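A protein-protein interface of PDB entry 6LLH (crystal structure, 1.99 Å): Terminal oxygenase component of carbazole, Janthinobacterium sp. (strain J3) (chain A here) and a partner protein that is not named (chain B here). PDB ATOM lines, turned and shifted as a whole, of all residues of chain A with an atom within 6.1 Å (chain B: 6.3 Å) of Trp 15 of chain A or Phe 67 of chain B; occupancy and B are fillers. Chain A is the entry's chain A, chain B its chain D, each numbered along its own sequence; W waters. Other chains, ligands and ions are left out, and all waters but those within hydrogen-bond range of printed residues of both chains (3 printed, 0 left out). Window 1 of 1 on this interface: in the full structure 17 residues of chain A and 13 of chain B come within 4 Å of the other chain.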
ATOM      1  N   LEU A   9      25.107 -21.016  13.436  1.00  0.00           N
ATOM      2  CA  LEU A   9      23.958 -20.774  14.322  1.00  0.00           C
ATOM      3  C   LEU A   9      23.897 -21.810  15.425  1.00  0.00           C
ATOM      4  O   LEU A   9      23.510 -21.452  16.579  1.00  0.00           O
ATOM      5  CB  LEU A   9      22.640 -20.756  13.550  1.00  0.00           C
ATOM      6  CG  LEU A   9      22.534 -19.654  12.524  1.00  0.00           C
ATOM      7  CD1 LEU A   9      21.232 -19.792  11.733  1.00  0.00           C
ATOM      8  CD2 LEU A   9      22.640 -18.278  13.164  1.00  0.00           C
ATOM      9  N   ARG A  11      26.406 -23.103  17.005  1.00  0.00           N
ATOM     10  CA  ARG A  11      27.408 -22.746  18.038  1.00  0.00           C
ATOM     11  C   ARG A  11      26.929 -21.607  18.950  1.00  0.00           C
ATOM     12  O   ARG A  11      27.321 -21.539  20.094  1.00  0.00           O
ATOM     13  CB  ARG A  11      28.726 -22.349  17.375  1.00  0.00           C
ATOM     14  CG  ARG A  11      29.601 -23.539  17.011  1.00  0.00           C
ATOM     15  CD  ARG A  11      30.735 -23.117  16.127  1.00  0.00           C
ATOM     16  NE  ARG A  11      31.793 -24.098  16.118  1.00  0.00           N
ATOM     17  CZ  ARG A  11      32.656 -24.323  17.114  1.00  0.00           C
ATOM     18  NH1 ARG A  11      32.654 -23.568  18.206  1.00  0.00           N
ATOM     19  NH2 ARG A  11      33.511 -25.337  17.002  1.00  0.00           N
ATOM     20  N   VAL A  12      26.136 -20.671  18.424  1.00  0.00           N
ATOM     21  CA  VAL A  12      25.797 -19.448  19.191  1.00  0.00           C
ATOM     22  C   VAL A  12      24.404 -19.601  19.819  1.00  0.00           C
ATOM     23  O   VAL A  12      23.469 -18.904  19.478  1.00  0.00           O
ATOM     24  CB  VAL A  12      25.895 -18.184  18.320  1.00  0.00           C
ATOM     25  CG1 VAL A  12      27.329 -17.858  17.966  1.00  0.00           C
ATOM     26  CG2 VAL A  12      25.062 -18.265  17.047  1.00  0.00           C
ATOM     27  N   LYS A  13      24.298 -20.507  20.777  1.00  0.00           N
ATOM     28  CA  LYS A  13      23.051 -20.918  21.368  1.00  0.00           C
ATOM     29  C   LYS A  13      22.432 -19.778  22.185  1.00  0.00           C
ATOM     30  O   LYS A  13      21.256 -19.751  22.375  1.00  0.00           O
ATOM     31  CB  LYS A  13      23.288 -22.110  22.296  1.00  0.00           C
ATOM     32  CG  LYS A  13      23.682 -23.392  21.586  1.00  0.00           C
ATOM     33  CD  LYS A  13      23.876 -24.563  22.527  1.00  0.00           C
ATOM     34  CE  LYS A  13      24.047 -25.862  21.764  1.00  0.00           C
ATOM     35  NZ  LYS A  13      25.144 -25.736  20.776  1.00  0.00           N
ATOM     36  N   GLY A  14      23.253 -18.860  22.702  1.00  0.00           N
ATOM     37  CA  GLY A  14      22.737 -17.695  23.456  1.00  0.00           C
ATOM     38  C   GLY A  14      21.877 -16.749  22.604  1.00  0.00           C
ATOM     39  O   GLY A  14      21.054 -16.012  23.137  1.00  0.00           O
ATOM     40  N   TRP A  15      22.099 -16.716  21.283  1.00  0.00           N
ATOM     41  CA  TRP A  15      21.573 -15.612  20.509  1.00  0.00           C
ATOM     42  C   TRP A  15      21.586 -15.894  19.012  1.00  0.00           C
ATOM     43  O   TRP A  15      21.850 -15.005  18.167  1.00  0.00           O
ATOM     44  CB  TRP A  15      22.324 -14.318  20.873  1.00  0.00           C
ATOM     45  CG  TRP A  15      23.819 -14.388  20.830  1.00  0.00           C
ATOM     46  CD1 TRP A  15      24.614 -14.313  19.727  1.00  0.00           C
ATOM     47  CD2 TRP A  15      24.708 -14.385  21.956  1.00  0.00           C
ATOM     48  NE1 TRP A  15      25.938 -14.317  20.085  1.00  0.00           N
ATOM     49  CE2 TRP A  15      26.023 -14.386  21.447  1.00  0.00           C
ATOM     50  CE3 TRP A  15      24.520 -14.339  23.341  1.00  0.00           C
ATOM     51  CZ2 TRP A  15      27.155 -14.372  22.272  1.00  0.00           C
ATOM     52  CZ3 TRP A  15      25.634 -14.388  24.150  1.00  0.00           C
ATOM     53  CH2 TRP A  15      26.932 -14.342  23.629  1.00  0.00           C
ATOM     54  N   ALA A  16      21.186 -17.112  18.650  1.00  0.00           N
ATOM     55  CA  ALA A  16      21.164 -17.540  17.251  1.00  0.00           C
ATOM     56  C   ALA A  16      20.228 -16.665  16.421  1.00  0.00           C
ATOM     57  O   ALA A  16      20.586 -16.287  15.311  1.00  0.00           O
ATOM     58  CB  ALA A  16      20.798 -19.014  17.135  1.00  0.00           C
ATOM     59  N   PRO A  17      19.005 -16.301  16.855  1.00  0.00           N
ATOM     60  CA  PRO A  17      18.140 -15.448  16.031  1.00  0.00           C
ATOM     61  C   PRO A  17      18.766 -14.090  15.705  1.00  0.00           C
ATOM     62  O   PRO A  17      18.650 -13.635  14.608  1.00  0.00           O
ATOM     63  CB  PRO A  17      16.858 -15.298  16.865  1.00  0.00           C
ATOM     64  CG  PRO A  17      16.852 -16.562  17.688  1.00  0.00           C
ATOM     65  CD  PRO A  17      18.318 -16.738  18.076  1.00  0.00           C
ATOM     66  N   TYR A  18      19.544 -13.527  16.627  1.00  0.00           N
ATOM     67  CA  TYR A  18      20.204 -12.256  16.401  1.00  0.00           C
ATOM     68  C   TYR A  18      21.314 -12.376  15.361  1.00  0.00           C
ATOM     69  O   TYR A  18      21.458 -11.537  14.485  1.00  0.00           O
ATOM     70  CB  TYR A  18      20.812 -11.769  17.718  1.00  0.00           C
ATOM     71  CG  TYR A  18      21.621 -10.503  17.629  1.00  0.00           C
ATOM     72  CD1 TYR A  18      21.015  -9.267  17.510  1.00  0.00           C
ATOM     73  CD2 TYR A  18      22.996 -10.543  17.733  1.00  0.00           C
ATOM     74  CE1 TYR A  18      21.761  -8.084  17.472  1.00  0.00           C
ATOM     75  CE2 TYR A  18      23.758  -9.383  17.692  1.00  0.00           C
ATOM     76  CZ  TYR A  18      23.141  -8.148  17.598  1.00  0.00           C
ATOM     77  OH  TYR A  18      23.904  -6.994  17.625  1.00  0.00           O
ATOM     78  N   VAL A  19      22.093 -13.453  15.447  1.00  0.00           N
ATOM     79  CA  VAL A  19      23.153 -13.706  14.518  1.00  0.00           C
ATOM     80  C   VAL A  19      22.539 -13.958  13.126  1.00  0.00           C
ATOM     81  O   VAL A  19      23.119 -13.593  12.092  1.00  0.00           O
ATOM     82  CB  VAL A  19      24.045 -14.866  15.012  1.00  0.00           C
ATOM     83  CG1 VAL A  19      25.050 -15.282  13.971  1.00  0.00           C
ATOM     84  CG2 VAL A  19      24.781 -14.489  16.274  1.00  0.00           C
ATOM     85  N   ASP A  20      21.352 -14.563  13.108  1.00  0.00           N
ATOM     86  CA  ASP A  20      20.647 -14.862  11.873  1.00  0.00           C
ATOM     87  C   ASP A  20      20.060 -13.584  11.254  1.00  0.00           C
ATOM     88  O   ASP A  20      19.813 -13.523  10.022  1.00  0.00           O
ATOM     89  CB  ASP A  20      19.499 -15.849  12.112  1.00  0.00           C
ATOM     90  CG  ASP A  20      19.085 -16.617  10.866  1.00  0.00           C
ATOM     91  OD1 ASP A  20      19.936 -16.822   9.993  1.00  0.00           O
ATOM     92  OD2 ASP A  20      17.919 -17.012  10.794  1.00  0.00           O
ATOM     93  N   TRP A 350      31.318 -13.881  14.952  1.00  0.00           N
ATOM     94  CA  TRP A 350      30.326 -14.218  15.954  1.00  0.00           C
ATOM     95  C   TRP A 350      30.745 -15.424  16.799  1.00  0.00           C
ATOM     96  O   TRP A 350      30.154 -15.651  17.851  1.00  0.00           O
ATOM     97  CB  TRP A 350      28.959 -14.500  15.325  1.00  0.00           C
ATOM     98  CG  TRP A 350      28.394 -13.365  14.564  1.00  0.00           C
ATOM     99  CD1 TRP A 350      28.213 -13.309  13.215  1.00  0.00           C
ATOM    100  CD2 TRP A 350      27.916 -12.119  15.083  1.00  0.00           C
ATOM    101  NE1 TRP A 350      27.677 -12.094  12.857  1.00  0.00           N
ATOM    102  CE2 TRP A 350      27.434 -11.369  13.979  1.00  0.00           C
ATOM    103  CE3 TRP A 350      27.826 -11.550  16.367  1.00  0.00           C
ATOM    104  CZ2 TRP A 350      26.942 -10.072  14.109  1.00  0.00           C
ATOM    105  CZ3 TRP A 350      27.307 -10.283  16.497  1.00  0.00           C
ATOM    106  CH2 TRP A 350      26.855  -9.568  15.392  1.00  0.00           C
ATOM    107  N   GLU A 353      35.259 -13.918  18.234  1.00  0.00           N
ATOM    108  CA  GLU A 353      35.423 -12.753  19.142  1.00  0.00           C
ATOM    109  C   GLU A 353      35.847 -13.232  20.545  1.00  0.00           C
ATOM    110  O   GLU A 353      35.360 -14.257  21.042  1.00  0.00           O
ATOM    111  CB  GLU A 353      34.099 -11.970  19.158  1.00  0.00           C
ATOM    112  CG  GLU A 353      32.919 -12.780  19.722  1.00  0.00           C
ATOM    113  CD  GLU A 353      31.522 -12.166  19.680  1.00  0.00           C
ATOM    114  OE1 GLU A 353      31.346 -11.155  19.003  1.00  0.00           O
ATOM    115  OE2 GLU A 353      30.586 -12.755  20.303  1.00  0.00           O
ATOM    116  N   LEU A 355      35.441 -11.833  24.170  1.00  0.00           N
ATOM    117  CA  LEU A 355      34.722 -10.833  24.944  1.00  0.00           C
ATOM    118  C   LEU A 355      35.436 -10.610  26.294  1.00  0.00           C
ATOM    119  O   LEU A 355      36.133 -11.508  26.789  1.00  0.00           O
ATOM    120  CB  LEU A 355      33.290 -11.323  25.173  1.00  0.00           C
ATOM    121  CG  LEU A 355      32.501 -11.516  23.887  1.00  0.00           C
ATOM    122  CD1 LEU A 355      31.039 -11.704  24.176  1.00  0.00           C
ATOM    123  CD2 LEU A 355      32.706 -10.366  22.911  1.00  0.00           C
ATOM    124  N   GLU A 360      29.227  -7.579  28.880  1.00  0.00           N
ATOM    125  CA  GLU A 360      27.960  -8.093  29.485  1.00  0.00           C
ATOM    126  C   GLU A 360      26.770  -7.294  28.952  1.00  0.00           C
ATOM    127  O   GLU A 360      25.711  -7.835  28.804  1.00  0.00           O
ATOM    128  CB  GLU A 360      27.913  -7.977  31.017  1.00  0.00           C
ATOM    129  CG  GLU A 360      28.803  -8.964  31.747  1.00  0.00           C
ATOM    130  CD  GLU A 360      28.439 -10.443  31.604  1.00  0.00           C
ATOM    131  OE1 GLU A 360      27.285 -10.732  31.092  1.00  0.00           O
ATOM    132  OE2 GLU A 360      29.293 -11.316  32.035  1.00  0.00           O
ATOM    133  N   VAL A 363      26.027  -8.680  25.441  1.00  0.00           N
ATOM    134  CA  VAL A 363      25.442 -10.000  25.631  1.00  0.00           C
ATOM    135  C   VAL A 363      23.968  -9.887  26.053  1.00  0.00           C
ATOM    136  O   VAL A 363      23.164 -10.614  25.516  1.00  0.00           O
ATOM    137  CB  VAL A 363      26.262 -10.847  26.614  1.00  0.00           C
ATOM    138  CG1 VAL A 363      25.502 -12.082  27.089  1.00  0.00           C
ATOM    139  CG2 VAL A 363      27.576 -11.277  25.976  1.00  0.00           C
ATOM    140  N   ARG A 366      22.065  -8.893  22.931  1.00  0.00           N
ATOM    141  CA  ARG A 366      21.925  -9.978  21.950  1.00  0.00           C
ATOM    142  C   ARG A 366      20.828 -10.958  22.386  1.00  0.00           C
ATOM    143  O   ARG A 366      20.050 -11.464  21.552  1.00  0.00           O
ATOM    144  CB  ARG A 366      23.260 -10.672  21.778  1.00  0.00           C
ATOM    145  CG  ARG A 366      24.324  -9.818  21.106  1.00  0.00           C
ATOM    146  CD  ARG A 366      25.618 -10.573  21.010  1.00  0.00           C
ATOM    147  NE  ARG A 366      26.716  -9.896  20.342  1.00  0.00           N
ATOM    148  CZ  ARG A 366      27.958 -10.388  20.244  1.00  0.00           C
ATOM    149  NH1 ARG A 366      28.221 -11.586  20.766  1.00  0.00           N
ATOM    150  NH2 ARG A 366      28.915  -9.659  19.672  1.00  0.00           N
ATOM    151  N   LYS A 367      20.783 -11.240  23.684  1.00  0.00           N
ATOM    152  CA  LYS A 367      19.776 -12.152  24.244  1.00  0.00           C
ATOM    153  C   LYS A 367      18.392 -11.510  24.214  1.00  0.00           C
ATOM    154  O   LYS A 367      17.416 -12.157  23.790  1.00  0.00           O
ATOM    155  CB  LYS A 367      20.150 -12.565  25.663  1.00  0.00           C
ATOM    156  CG  LYS A 367      21.410 -13.390  25.693  1.00  0.00           C
ATOM    157  CD  LYS A 367      21.682 -14.127  26.958  1.00  0.00           C
ATOM    158  CE  LYS A 367      22.872 -15.050  26.785  1.00  0.00           C
ATOM    159  NZ  LYS A 367      23.121 -15.846  28.012  1.00  0.00           N
ATOM    160  N   SER A 370      17.275 -11.472  20.667  1.00  0.00           N
ATOM    161  CA  SER A 370      16.954 -12.792  20.226  1.00  0.00           C
ATOM    162  C   SER A 370      15.598 -13.223  20.762  1.00  0.00           C
ATOM    163  O   SER A 370      14.935 -13.953  20.087  1.00  0.00           O
ATOM    164  CB  SER A 370      17.981 -13.824  20.612  1.00  0.00           C
ATOM    165  OG  SER A 370      19.227 -13.548  19.990  1.00  0.00           O
ATOM    166  N   GLY B  49      36.072 -16.038  26.902  1.00  0.00           N
ATOM    167  CA  GLY B  49      35.220 -14.865  26.991  1.00  0.00           C
ATOM    168  C   GLY B  49      34.682 -14.668  28.390  1.00  0.00           C
ATOM    169  O   GLY B  49      35.457 -14.567  29.343  1.00  0.00           O
ATOM    170  N   ILE B  50      33.365 -14.517  28.504  1.00  0.00           N
ATOM    171  CA  ILE B  50      32.745 -14.232  29.806  1.00  0.00           C
ATOM    172  C   ILE B  50      31.546 -15.150  30.051  1.00  0.00           C
ATOM    173  O   ILE B  50      30.762 -14.893  30.960  1.00  0.00           O
ATOM    174  CB  ILE B  50      32.345 -12.743  29.910  1.00  0.00           C
ATOM    175  CG1 ILE B  50      31.428 -12.318  28.761  1.00  0.00           C
ATOM    176  CG2 ILE B  50      33.603 -11.864  30.021  1.00  0.00           C
ATOM    177  CD1 ILE B  50      30.786 -10.945  28.959  1.00  0.00           C
ATOM    178  N   ALA B  51      31.390 -16.202  29.230  1.00  0.00           N
ATOM    179  CA  ALA B  51      30.264 -17.159  29.398  1.00  0.00           C
ATOM    180  C   ALA B  51      30.367 -17.915  30.737  1.00  0.00           C
ATOM    181  O   ALA B  51      31.467 -18.248  31.207  1.00  0.00           O
ATOM    182  CB  ALA B  51      30.307 -18.145  28.257  1.00  0.00           C
ATOM    183  N   SER B  52      29.211 -18.284  31.287  1.00  0.00           N
ATOM    184  CA  SER B  52      29.129 -19.259  32.381  1.00  0.00           C
ATOM    185  C   SER B  52      28.956 -20.697  31.843  1.00  0.00           C
ATOM    186  O   SER B  52      27.885 -21.078  31.332  1.00  0.00           O
ATOM    187  CB  SER B  52      28.006 -18.907  33.305  1.00  0.00           C
ATOM    188  OG  SER B  52      27.802 -19.981  34.213  1.00  0.00           O
ATOM    189  N   GLU B  55      26.008 -23.022  32.358  1.00  0.00           N
ATOM    190  CA  GLU B  55      24.856 -22.899  31.508  1.00  0.00           C
ATOM    191  C   GLU B  55      25.104 -23.649  30.206  1.00  0.00           C
ATOM    192  O   GLU B  55      24.361 -23.501  29.298  1.00  0.00           O
ATOM    193  CB  GLU B  55      24.531 -21.427  31.269  1.00  0.00           C
ATOM    194  CG  GLU B  55      24.259 -20.689  32.566  1.00  0.00           C
ATOM    195  CD  GLU B  55      23.928 -19.217  32.402  1.00  0.00           C
ATOM    196  OE1 GLU B  55      23.845 -18.757  31.241  1.00  0.00           O
ATOM    197  OE2 GLU B  55      23.739 -18.531  33.440  1.00  0.00           O
ATOM    198  N   CYS B  65      30.608 -24.709  25.761  1.00  0.00           N
ATOM    199  CA  CYS B  65      30.284 -23.356  26.186  1.00  0.00           C
ATOM    200  C   CYS B  65      29.065 -22.854  25.412  1.00  0.00           C
ATOM    201  O   CYS B  65      29.004 -23.011  24.197  1.00  0.00           O
ATOM    202  CB  CYS B  65      31.474 -22.421  25.961  1.00  0.00           C
ATOM    203  SG  CYS B  65      31.054 -20.690  26.287  1.00  0.00           S
ATOM    204  N   PRO B  66      28.099 -22.188  26.087  1.00  0.00           N
ATOM    205  CA  PRO B  66      26.863 -21.714  25.453  1.00  0.00           C
ATOM    206  C   PRO B  66      27.001 -20.516  24.493  1.00  0.00           C
ATOM    207  O   PRO B  66      26.124 -20.321  23.590  1.00  0.00           O
ATOM    208  CB  PRO B  66      25.969 -21.350  26.667  1.00  0.00           C
ATOM    209  CG  PRO B  66      26.928 -21.005  27.753  1.00  0.00           C
ATOM    210  CD  PRO B  66      28.112 -21.921  27.535  1.00  0.00           C
ATOM    211  N   PHE B  67      28.116 -19.768  24.607  1.00  0.00           N
ATOM    212  CA  PHE B  67      28.315 -18.584  23.805  1.00  0.00           C
ATOM    213  C   PHE B  67      28.741 -18.937  22.385  1.00  0.00           C
ATOM    214  O   PHE B  67      28.069 -18.483  21.457  1.00  0.00           O
ATOM    215  CB  PHE B  67      29.349 -17.648  24.425  1.00  0.00           C
ATOM    216  CG  PHE B  67      28.822 -16.686  25.453  1.00  0.00           C
ATOM    217  CD1 PHE B  67      27.643 -16.937  26.147  1.00  0.00           C
ATOM    218  CD2 PHE B  67      29.536 -15.533  25.756  1.00  0.00           C
ATOM    219  CE1 PHE B  67      27.198 -16.063  27.132  1.00  0.00           C
ATOM    220  CE2 PHE B  67      29.065 -14.644  26.708  1.00  0.00           C
ATOM    221  CZ  PHE B  67      27.924 -14.926  27.422  1.00  0.00           C
ATOM    222  N   HIS B  68      29.872 -19.654  22.216  1.00  0.00           N
ATOM    223  CA  HIS B  68      30.456 -19.845  20.877  1.00  0.00           C
ATOM    224  C   HIS B  68      30.649 -21.324  20.518  1.00  0.00           C
ATOM    225  O   HIS B  68      31.169 -21.611  19.466  1.00  0.00           O
ATOM    226  CB  HIS B  68      31.775 -19.075  20.757  1.00  0.00           C
ATOM    227  CG  HIS B  68      31.626 -17.623  21.075  1.00  0.00           C
ATOM    228  ND1 HIS B  68      32.285 -17.031  22.125  1.00  0.00           N
ATOM    229  CD2 HIS B  68      30.878 -16.648  20.494  1.00  0.00           C
ATOM    230  CE1 HIS B  68      31.923 -15.758  22.216  1.00  0.00           C
ATOM    231  NE2 HIS B  68      31.112 -15.479  21.185  1.00  0.00           N
ATOM    232  N   GLY B  69      30.232 -22.254  21.381  1.00  0.00           N
ATOM    233  CA  GLY B  69      30.413 -23.703  21.133  1.00  0.00           C
ATOM    234  C   GLY B  69      31.837 -24.228  21.339  1.00  0.00           C
ATOM    235  O   GLY B  69      32.114 -25.367  20.994  1.00  0.00           O
ATOM    236  N   GLY B  70      32.747 -23.413  21.893  1.00  0.00           N
ATOM    237  CA  GLY B  70      34.000 -23.934  22.475  1.00  0.00           C
ATOM    238  C   GLY B  70      33.729 -24.968  23.553  1.00  0.00           C
ATOM    239  O   GLY B  70      32.621 -25.049  24.105  1.00  0.00           O
HETATM  240  O   HOH W   1      24.424 -18.298  28.487  1.00  0.00           O
HETATM  241  O   HOH W   2      27.306 -23.718  22.109  1.00  0.00           O
HETATM  242  O   HOH W   3      25.596 -17.413  21.879  1.00  0.00           O
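Of the 19 printed residues of chain A, 10 touch a printed residue of chain B. Hydrophobic or aromatic side chains of chain A within 4 Å of the printed part of chain B: Val 12, Trp 15 and Val 363. Among the printed residues, 14 pairs touch across the chains. Among the printed residues, no Asp or Glu carboxylate lies within 4 Å of a Lys or Arg side-chain nitrogen of the other chain.
Of chain B, only Phe 67 comes within 4 Å of Trp 15 of chain A. Phe 67 of chain B touches just these residues of chain A: Arg 11, Val 12, Trp 15 and Val 363. Printed residues of chain A within 4 Å of Ile 50 of chain B: Glu 360 (3.4 Å). Of the printed residues of chain A, Gly 49 of chain B touches Leu 355. Printed residues of chain B within 4 Å of Gly 14 of chain A: Pro 66. Glu 55 of chain B touches none of the printed residues of chain A. Asp 20 of chain A touches none of the printed residues of chain B. The nearest residue of chain B that does not touch Trp 15 of chain A is His 68 of chain B (4.3 Å). The nearest printed residue of chain B that does not touch Val 12 of chain A is Pro 66 of chain B (4.2 Å).
The guanidinium group (NH1) of Arg 11 of chain A sits at hydrogen-bond distance from the backbone carbonyl oxygen (O) of His 68 of chain B, 2.8 Å away. The backbone NH of Gly 69 of chain B sits at hydrogen-bond distance from the backbone carbonyl oxygen of Arg 11 of chain A, at 3.3 Å. The backbone NH of Lys 13 of chain A sits at hydrogen-bond distance from the backbone carbonyl oxygen of Pro 66 of chain B (3.4 Å). N of Gly 14 of chain A sits at hydrogen-bond distance from O of Pro 66 of chain B (3.3 Å). The backbone carbonyl oxygen of Trp 350 of chain A sits close to a ring nitrogen (NE2) of His 68 of chain B. OE2 of Glu 353 of chain A lies within hydrogen-bond range of NE2 of His 68 of chain B, at 2.9 Å. The backbone carbonyl oxygen of Arg 11 of chain A lies close to the backbone carbonyl oxygen of Phe 67 of chain B, at 3.4 Å.
OE2 of Glu 353 of chain A is in salt-bridge range of NH1 of Arg 366 of chain A (2.7 Å). The backbone NH (N) of Phe 67 of chain B lies close to the side-chain sulfur (SG) of Cys 65 of chain B (3.5 Å). The backbone NH (N) of Cys 65 of chain B lies within hydrogen-bond range of the backbone carbonyl oxygen (O) of Gly 70 of chain B (2.6 Å).
Water W3 lies within hydrogen-bond range of O of Phe 67 of chain B (2.7 Å), N of Gly 14 of chain A (2.9 Å) and O of Pro 66 of chain B (3.4 Å). Water W2 lies within hydrogen-bond range of the backbone carbonyl oxygen of Cys 65 of chain B (2.8 Å), the backbone carbonyl oxygen of Arg 11 of chain A (3.0 Å), the side-chain amino group of Lys 13 of chain A (3.2 Å) and the backbone NH of Gly 69 of chain B (3.4 Å). Water W1 lies within hydrogen-bond range of NZ of Lys 367 of chain A and OE1 of Glu 55 of chain B.
Among the printed residues, merely in contact across the chains: Val 12 of chain A with Phe 67 of chain B, Glu 360 of chain A with Ile 50 of chain B, Leu 355 of chain A with Gly 49 of chain B, Trp 15 of chain A with Phe 67 of chain B, Arg 11 of chain A with Gly 70 of chain B, Val 363 of chain A with Phe 67 of chain B and Arg 11 of chain A with Pro 66 of chain B.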
